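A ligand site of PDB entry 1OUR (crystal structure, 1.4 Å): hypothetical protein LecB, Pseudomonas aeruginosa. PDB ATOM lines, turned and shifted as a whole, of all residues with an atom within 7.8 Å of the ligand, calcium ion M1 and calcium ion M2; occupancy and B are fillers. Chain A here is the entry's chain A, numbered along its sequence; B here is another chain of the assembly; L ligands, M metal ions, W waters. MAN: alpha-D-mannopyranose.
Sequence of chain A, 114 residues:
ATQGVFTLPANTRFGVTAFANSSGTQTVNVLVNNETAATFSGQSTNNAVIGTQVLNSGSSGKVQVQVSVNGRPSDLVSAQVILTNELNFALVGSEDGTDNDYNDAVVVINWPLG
O4 of the ligand sits close to OD1 of Asp 96 (2.7 Å).
OG of Ser 23 sits at hydrogen-bond distance from O6 of the ligand (2.6 Å).
An oxygen (O5) of the ligand is in hydrogen-bond range of the backbone NH (N) of Ser 23, 3.1 Å away.
Four residues have an atom within 4 Å of calcium ion M1: Glu 95, Asp 99, Asp 101 and Asp 104.
The nearest printed residue that does not touch calcium ion M2 is Ser 22 (4.4 Å).
N of Asn 103 lies within hydrogen-bond range of O of Ser 94 (3.4 Å).
OD2 of Asp 96 lies within hydrogen-bond range of OG of Ser 22.
O of Pro 112 of chain B sits at hydrogen-bond distance from ND2 of Asn 103.
The backbone NH (N) of Ser 22 sits at hydrogen-bond distance from the backbone carbonyl oxygen (O) of Ser 44, 2.8 Å away.
The side-chain amide oxygen (OE1) of Gln 26 lies close to the side-chain carboxylate (OD2) of Asp 96 (3.1 Å).
OE1 of Glu 95 lies close to N of Asn 100, at 3.4 Å.
The side-chain carboxylate of Asp 104 sits close to the backbone NH of Asp 96.
OE2 of Glu 95 lies close to N of Gly 97 (2.7 Å).
Calcium ion M1 is bound by OE2 of Glu 95 (2.4 Å).
OD1 of Asp 101 binds calcium ion M1, 2.4 Å away.
Calcium ion M1 is bound by the side-chain carboxylate (OD1) of Asp 99 (2.4 Å).
OD2 of Asp 104 is bound to calcium ion M1 (2.4 Å).
The side-chain carboxylate (OE1) of Glu 95 binds calcium ion M1, 2.5 Å away.
O3 of the ligand binds calcium ion M1 (2.5 Å).
OD1 of Asp 104 is bound to calcium ion M1 (2.6 Å).
Calcium ion M1 is bound by O4 of the ligand (2.7 Å).
OD1 of Asn 103 is bound to calcium ion M2, at 2.4 Å.
Calcium ion M2 is bound by O of Asn 21.
Calcium ion M2 is bound by OD2 of Asp 101 (2.4 Å).
An oxygen (O3) of the ligand is bound to calcium ion M2 (2.4 Å).
O2 of the ligand is bound to calcium ion M2, 2.4 Å away.
OD1 of Asp 104 is bound to calcium ion M2, at 2.4 Å.
The chain-end carboxylate (O) of Gly 114 of chain B binds calcium ion M2.
Slightly farther from calcium ion M2 lies the side-chain carboxylate (OD1) of Asp 101 (3.1 Å).
Merely in contact with the ligand: Ser 22, Thr 45 and Gly 97.
Of the 26 residues printed, 11 come within 4 Å of the ligand.
The nearest printed residue that does not touch the ligand is Asn 103 (4.4 Å).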
ATOM      1  N   ALA A  20       0.319  21.240  19.790  1.00  0.00           N
ATOM      2  CA  ALA A  20       1.083  21.584  20.984  1.00  0.00           C
ATOM      3  C   ALA A  20       2.130  20.528  21.315  1.00  0.00           C
ATOM      4  O   ALA A  20       1.886  19.328  21.171  1.00  0.00           O
ATOM      5  CB  ALA A  20       0.153  21.790  22.169  1.00  0.00           C
ATOM      6  N   ASN A  21       3.302  20.989  21.752  1.00  0.00           N
ATOM      7  CA  ASN A  21       4.422  20.133  22.127  1.00  0.00           C
ATOM      8  C   ASN A  21       5.173  20.830  23.249  1.00  0.00           C
ATOM      9  O   ASN A  21       6.277  21.323  23.047  1.00  0.00           O
ATOM     10  CB  ASN A  21       5.366  19.925  20.940  1.00  0.00           C
ATOM     11  CG  ASN A  21       4.741  19.084  19.848  1.00  0.00           C
ATOM     12  OD1 ASN A  21       4.629  17.863  19.977  1.00  0.00           O
ATOM     13  ND2 ASN A  21       4.324  19.733  18.768  1.00  0.00           N
ATOM     14  N   SER A  22       4.572  20.871  24.428  1.00  0.00           N
ATOM     15  CA  SER A  22       5.176  21.548  25.574  1.00  0.00           C
ATOM     16  C   SER A  22       4.448  21.234  26.872  1.00  0.00           C
ATOM     17  O   SER A  22       3.280  20.835  26.854  1.00  0.00           O
ATOM     18  CB  SER A  22       5.161  23.062  25.340  1.00  0.00           C
ATOM     19  OG  SER A  22       5.575  23.762  26.504  1.00  0.00           O
ATOM     20  N   SER A  23       5.140  21.405  27.988  1.00  0.00           N
ATOM     21  CA  SER A  23       4.539  21.164  29.292  1.00  0.00           C
ATOM     22  C   SER A  23       3.569  22.311  29.571  1.00  0.00           C
ATOM     23  O   SER A  23       2.590  22.142  30.305  1.00  0.00           O
ATOM     24  CB  SER A  23       5.606  21.130  30.380  1.00  0.00           C
ATOM     25  OG  SER A  23       6.247  22.386  30.496  1.00  0.00           O
ATOM     26  N   GLY A  24       3.841  23.474  28.992  1.00  0.00           N
ATOM     27  CA  GLY A  24       2.995  24.620  29.218  1.00  0.00           C
ATOM     28  C   GLY A  24       1.756  24.688  28.343  1.00  0.00           C
ATOM     29  O   GLY A  24       1.760  24.243  27.199  1.00  0.00           O
ATOM     30  N   THR A  25       0.694  25.268  28.891  1.00  0.00           N
ATOM     31  CA  THR A  25      -0.553  25.430  28.168  1.00  0.00           C
ATOM     32  C   THR A  25      -0.332  26.500  27.104  1.00  0.00           C
ATOM     33  O   THR A  25       0.094  27.614  27.412  1.00  0.00           O
ATOM     34  CB  THR A  25      -1.681  25.868  29.108  1.00  0.00           C
ATOM     35  OG1 THR A  25      -1.892  24.837  30.086  1.00  0.00           O
ATOM     36  CG2 THR A  25      -2.976  26.108  28.339  1.00  0.00           C
ATOM     37  N   GLN A  26      -0.623  26.152  25.850  1.00  0.00           N
ATOM     38  CA  GLN A  26      -0.437  27.067  24.735  1.00  0.00           C
ATOM     39  C   GLN A  26      -1.692  27.848  24.398  1.00  0.00           C
ATOM     40  O   GLN A  26      -2.785  27.280  24.302  1.00  0.00           O
ATOM     41  CB  GLN A  26      -0.004  26.266  23.505  1.00  0.00           C
ATOM     42  CG  GLN A  26       1.205  25.381  23.742  1.00  0.00           C
ATOM     43  CD  GLN A  26       2.467  26.165  24.059  1.00  0.00           C
ATOM     44  OE1 GLN A  26       3.202  25.830  24.991  1.00  0.00           O
ATOM     45  NE2 GLN A  26       2.731  27.184  23.255  1.00  0.00           N
ATOM     46  N   GLN A  43      -2.967  21.842  25.874  1.00  0.00           N
ATOM     47  CA  GLN A  43      -1.682  21.365  26.346  1.00  0.00           C
ATOM     48  C   GLN A  43      -1.449  19.936  25.872  1.00  0.00           C
ATOM     49  O   GLN A  43      -2.335  19.093  25.947  1.00  0.00           O
ATOM     50  CB  GLN A  43      -1.630  21.434  27.878  1.00  0.00           C
ATOM     51  CG  GLN A  43      -0.296  21.048  28.538  1.00  0.00           C
ATOM     52  CD  GLN A  43       0.019  19.562  28.446  1.00  0.00           C
ATOM     53  OE1 GLN A  43      -0.834  18.720  28.731  1.00  0.00           O
ATOM     54  NE2 GLN A  43       1.264  19.239  28.095  1.00  0.00           N
ATOM     55  N   SER A  44      -0.240  19.693  25.368  1.00  0.00           N
ATOM     56  CA  SER A  44       0.150  18.383  24.881  1.00  0.00           C
ATOM     57  C   SER A  44       1.638  18.360  24.639  1.00  0.00           C
ATOM     58  O   SER A  44       2.250  19.386  24.329  1.00  0.00           O
ATOM     59  CB  SER A  44      -0.570  18.063  23.564  1.00  0.00           C
ATOM     60  OG  SER A  44      -0.113  16.830  23.023  1.00  0.00           O
ATOM     61  N   THR A  45       2.242  17.192  24.821  1.00  0.00           N
ATOM     62  CA  THR A  45       3.662  17.010  24.554  1.00  0.00           C
ATOM     63  C   THR A  45       3.749  15.931  23.480  1.00  0.00           C
ATOM     64  O   THR A  45       4.826  15.379  23.230  1.00  0.00           O
ATOM     65  CB  THR A  45       4.466  16.574  25.800  1.00  0.00           C
ATOM     66  OG1 THR A  45       3.775  15.506  26.468  1.00  0.00           O
ATOM     67  CG2 THR A  45       4.659  17.745  26.752  1.00  0.00           C
ATOM     68  N   VAL A  69       2.215  31.686  26.563  1.00  0.00           N
ATOM     69  CA  VAL A  69       2.084  30.672  27.607  1.00  0.00           C
ATOM     70  C   VAL A  69       1.965  31.447  28.911  1.00  0.00           C
ATOM     71  O   VAL A  69       2.869  32.203  29.275  1.00  0.00           O
ATOM     72  CB  VAL A  69       3.307  29.743  27.665  1.00  0.00           C
ATOM     73  CG1 VAL A  69       3.168  28.769  28.837  1.00  0.00           C
ATOM     74  CG2 VAL A  69       3.434  28.971  26.355  1.00  0.00           C
ATOM     75  N   SER A  94       6.901  28.195  17.455  1.00  0.00           N
ATOM     76  CA  SER A  94       7.046  29.076  18.606  1.00  0.00           C
ATOM     77  C   SER A  94       7.848  28.420  19.724  1.00  0.00           C
ATOM     78  O   SER A  94       7.789  27.203  19.911  1.00  0.00           O
ATOM     79  CB  SER A  94       5.667  29.492  19.137  1.00  0.00           C
ATOM     80  OG  SER A  94       4.928  28.357  19.545  1.00  0.00           O
ATOM     81  N   GLU A  95       8.600  29.237  20.441  1.00  0.00           N
ATOM     82  CA  GLU A  95       9.414  28.743  21.547  1.00  0.00           C
ATOM     83  C   GLU A  95       9.015  29.458  22.832  1.00  0.00           C
ATOM     84  O   GLU A  95       9.049  30.681  22.910  1.00  0.00           O
ATOM     85  CB  GLU A  95      10.896  28.990  21.255  1.00  0.00           C
ATOM     86  CG  GLU A  95      11.828  28.530  22.362  1.00  0.00           C
ATOM     87  CD  GLU A  95      11.613  27.075  22.731  1.00  0.00           C
ATOM     88  OE1 GLU A  95      11.637  26.222  21.829  1.00  0.00           O
ATOM     89  OE2 GLU A  95      11.433  26.791  23.932  1.00  0.00           O
ATOM     90  N   ASP A  96       8.625  28.662  23.832  1.00  0.00           N
ATOM     91  CA  ASP A  96       8.215  29.226  25.120  1.00  0.00           C
ATOM     92  C   ASP A  96       9.302  29.108  26.174  1.00  0.00           C
ATOM     93  O   ASP A  96       9.160  29.661  27.266  1.00  0.00           O
ATOM     94  CB  ASP A  96       6.939  28.531  25.637  1.00  0.00           C
ATOM     95  CG  ASP A  96       7.133  27.033  25.867  1.00  0.00           C
ATOM     96  OD1 ASP A  96       8.205  26.627  26.379  1.00  0.00           O
ATOM     97  OD2 ASP A  96       6.193  26.266  25.576  1.00  0.00           O
ATOM     98  N   GLY A  97      10.384  28.396  25.850  1.00  0.00           N
ATOM     99  CA  GLY A  97      11.429  28.206  26.831  1.00  0.00           C
ATOM    100  C   GLY A  97      12.862  28.405  26.383  1.00  0.00           C
ATOM    101  O   GLY A  97      13.194  29.377  25.710  1.00  0.00           O
ATOM    102  N   THR A  98      13.712  27.452  26.762  1.00  0.00           N
ATOM    103  CA  THR A  98      15.140  27.521  26.469  1.00  0.00           C
ATOM    104  C   THR A  98      15.727  26.415  25.593  1.00  0.00           C
ATOM    105  O   THR A  98      16.887  26.514  25.180  1.00  0.00           O
ATOM    106  CB  THR A  98      15.932  27.507  27.786  1.00  0.00           C
ATOM    107  OG1 THR A  98      15.622  26.308  28.509  1.00  0.00           O
ATOM    108  CG2 THR A  98      15.562  28.713  28.645  1.00  0.00           C
ATOM    109  N   ASP A  99      14.978  25.359  25.293  1.00  0.00           N
ATOM    110  CA  ASP A  99      15.529  24.260  24.501  1.00  0.00           C
ATOM    111  C   ASP A  99      15.542  24.535  22.996  1.00  0.00           C
ATOM    112  O   ASP A  99      16.156  23.803  22.227  1.00  0.00           O
ATOM    113  CB  ASP A  99      14.797  22.958  24.815  1.00  0.00           C
ATOM    114  CG  ASP A  99      13.371  22.929  24.296  1.00  0.00           C
ATOM    115  OD1 ASP A  99      12.812  24.004  24.014  1.00  0.00           O
ATOM    116  OD2 ASP A  99      12.821  21.813  24.185  1.00  0.00           O
ATOM    117  N   ASN A 100      14.860  25.598  22.594  1.00  0.00           N
ATOM    118  CA  ASN A 100      14.781  26.011  21.195  1.00  0.00           C
ATOM    119  C   ASN A 100      14.322  24.981  20.169  1.00  0.00           C
ATOM    120  O   ASN A 100      14.899  24.892  19.087  1.00  0.00           O
ATOM    121  CB  ASN A 100      16.129  26.589  20.744  1.00  0.00           C
ATOM    122  CG  ASN A 100      16.535  27.805  21.540  1.00  0.00           C
ATOM    123  OD1 ASN A 100      15.744  28.735  21.719  1.00  0.00           O
ATOM    124  ND2 ASN A 100      17.776  27.828  22.006  1.00  0.00           N
ATOM    125  N   ASP A 101      13.313  24.194  20.502  1.00  0.00           N
ATOM    126  CA  ASP A 101      12.826  23.242  19.516  1.00  0.00           C
ATOM    127  C   ASP A 101      11.759  23.913  18.655  1.00  0.00           C
ATOM    128  O   ASP A 101      11.368  23.394  17.618  1.00  0.00           O
ATOM    129  CB  ASP A 101      12.320  21.932  20.166  1.00  0.00           C
ATOM    130  CG  ASP A 101      11.203  22.142  21.174  1.00  0.00           C
ATOM    131  OD1 ASP A 101      10.813  23.296  21.455  1.00  0.00           O
ATOM    132  OD2 ASP A 101      10.721  21.115  21.716  1.00  0.00           O
ATOM    133  N   TYR A 102      11.321  25.100  19.096  1.00  0.00           N
ATOM    134  CA  TYR A 102      10.329  25.906  18.380  1.00  0.00           C
ATOM    135  C   TYR A 102       9.073  25.188  17.919  1.00  0.00           C
ATOM    136  O   TYR A 102       8.450  25.567  16.930  1.00  0.00           O
ATOM    137  CB  TYR A 102      11.001  26.613  17.202  1.00  0.00           C
ATOM    138  CG  TYR A 102      11.733  27.871  17.626  1.00  0.00           C
ATOM    139  CD1 TYR A 102      11.071  29.103  17.687  1.00  0.00           C
ATOM    140  CD2 TYR A 102      13.051  27.818  18.086  1.00  0.00           C
ATOM    141  CE1 TYR A 102      11.694  30.236  18.202  1.00  0.00           C
ATOM    142  CE2 TYR A 102      13.680  28.944  18.605  1.00  0.00           C
ATOM    143  CZ  TYR A 102      12.998  30.146  18.671  1.00  0.00           C
ATOM    144  OH  TYR A 102      13.605  31.260  19.206  1.00  0.00           O
ATOM    145  N   ASN A 103       8.681  24.157  18.670  1.00  0.00           N
ATOM    146  CA  ASN A 103       7.503  23.377  18.322  1.00  0.00           C
ATOM    147  C   ASN A 103       6.466  23.411  19.439  1.00  0.00           C
ATOM    148  O   ASN A 103       5.447  22.724  19.373  1.00  0.00           O
ATOM    149  CB  ASN A 103       7.893  21.914  18.110  1.00  0.00           C
ATOM    150  CG  ASN A 103       8.237  21.208  19.414  1.00  0.00           C
ATOM    151  OD1 ASN A 103       8.289  21.836  20.477  1.00  0.00           O
ATOM    152  ND2 ASN A 103       8.480  19.910  19.344  1.00  0.00           N
ATOM    153  N   ASP A 104       6.722  24.219  20.467  1.00  0.00           N
ATOM    154  CA  ASP A 104       5.820  24.285  21.607  1.00  0.00           C
ATOM    155  C   ASP A 104       4.375  24.509  21.173  1.00  0.00           C
ATOM    156  O   ASP A 104       3.451  23.919  21.730  1.00  0.00           O
ATOM    157  CB  ASP A 104       6.328  25.338  22.586  1.00  0.00           C
ATOM    158  CG  ASP A 104       7.767  25.062  23.010  1.00  0.00           C
ATOM    159  OD1 ASP A 104       8.080  23.870  23.239  1.00  0.00           O
ATOM    160  OD2 ASP A 104       8.582  25.996  23.108  1.00  0.00           O
ATOM    161  N   ALA A 105       4.219  25.355  20.169  1.00  0.00           N
ATOM    162  CA  ALA A 105       2.932  25.622  19.560  1.00  0.00           C
ATOM    163  C   ALA A 105       3.285  25.725  18.077  1.00  0.00           C
ATOM    164  O   ALA A 105       4.097  26.550  17.687  1.00  0.00           O
ATOM    165  CB  ALA A 105       2.337  26.922  20.055  1.00  0.00           C
ATOM    166  N   PRO B 112      10.610  18.454  15.034  1.00  0.00           N
ATOM    167  CA  PRO B 112      10.486  17.458  16.101  1.00  0.00           C
ATOM    168  C   PRO B 112       9.221  17.651  16.934  1.00  0.00           C
ATOM    169  O   PRO B 112       8.556  18.678  16.841  1.00  0.00           O
ATOM    170  CB  PRO B 112      11.744  17.708  16.921  1.00  0.00           C
ATOM    171  CG  PRO B 112      11.793  19.215  16.879  1.00  0.00           C
ATOM    172  CD  PRO B 112      11.655  19.427  15.380  1.00  0.00           C
ATOM    173  N   LEU B 113       8.919  16.646  17.753  1.00  0.00           N
ATOM    174  CA  LEU B 113       7.761  16.691  18.640  1.00  0.00           C
ATOM    175  C   LEU B 113       8.245  16.721  20.088  1.00  0.00           C
ATOM    176  O   LEU B 113       9.445  16.628  20.358  1.00  0.00           O
ATOM    177  CB  LEU B 113       6.878  15.451  18.447  1.00  0.00           C
ATOM    178  CG  LEU B 113       6.371  15.132  17.033  1.00  0.00           C
ATOM    179  CD1 LEU B 113       5.454  13.928  17.096  1.00  0.00           C
ATOM    180  CD2 LEU B 113       5.633  16.331  16.454  1.00  0.00           C
ATOM    181  N   GLY B 114       7.299  16.871  21.009  1.00  0.00           N
ATOM    182  CA  GLY B 114       7.599  16.880  22.429  1.00  0.00           C
ATOM    183  C   GLY B 114       7.995  18.220  23.028  1.00  0.00           C
ATOM    184  O   GLY B 114       8.330  19.157  22.277  1.00  0.00           O
ATOM    185  OXT GLY B 114       7.987  18.312  24.276  1.00  0.00           O
HETATM  186  C1  MAN L   1       8.933  20.647  27.409  1.00  0.00           C
HETATM  187  C2  MAN L   1       9.385  20.789  25.942  1.00  0.00           C
HETATM  188  C3  MAN L   1      10.080  22.140  25.706  1.00  0.00           C
HETATM  189  C4  MAN L   1       9.204  23.283  26.219  1.00  0.00           C
HETATM  190  C5  MAN L   1       8.945  23.017  27.692  1.00  0.00           C
HETATM  191  C6  MAN L   1       8.214  24.137  28.421  1.00  0.00           C
HETATM  192  O1  MAN L   1       8.134  19.535  27.533  1.00  0.00           O
HETATM  193  O2  MAN L   1       8.269  20.694  25.061  1.00  0.00           O
HETATM  194  O3  MAN L   1      10.343  22.329  24.330  1.00  0.00           O
HETATM  195  O4  MAN L   1       9.861  24.532  26.022  1.00  0.00           O
HETATM  196  O5  MAN L   1       8.185  21.803  27.830  1.00  0.00           O
HETATM  197  O6  MAN L   1       8.253  23.934  29.829  1.00  0.00           O
HETATM  198 CA    CA M   1      10.583  24.630  23.420  1.00  0.00          CA
HETATM  199 CA    CA M   2       8.629  21.530  22.803  1.00  0.00          CA
HETATM  200  O   HOH W   1       7.131  17.960  29.720  1.00  0.00           O
HETATM  201  O   HOH W   2       9.209  19.292  30.550  1.00  0.00           O
HETATM  202  O   HOH W   3      12.495  24.870  27.098  1.00  0.00           O
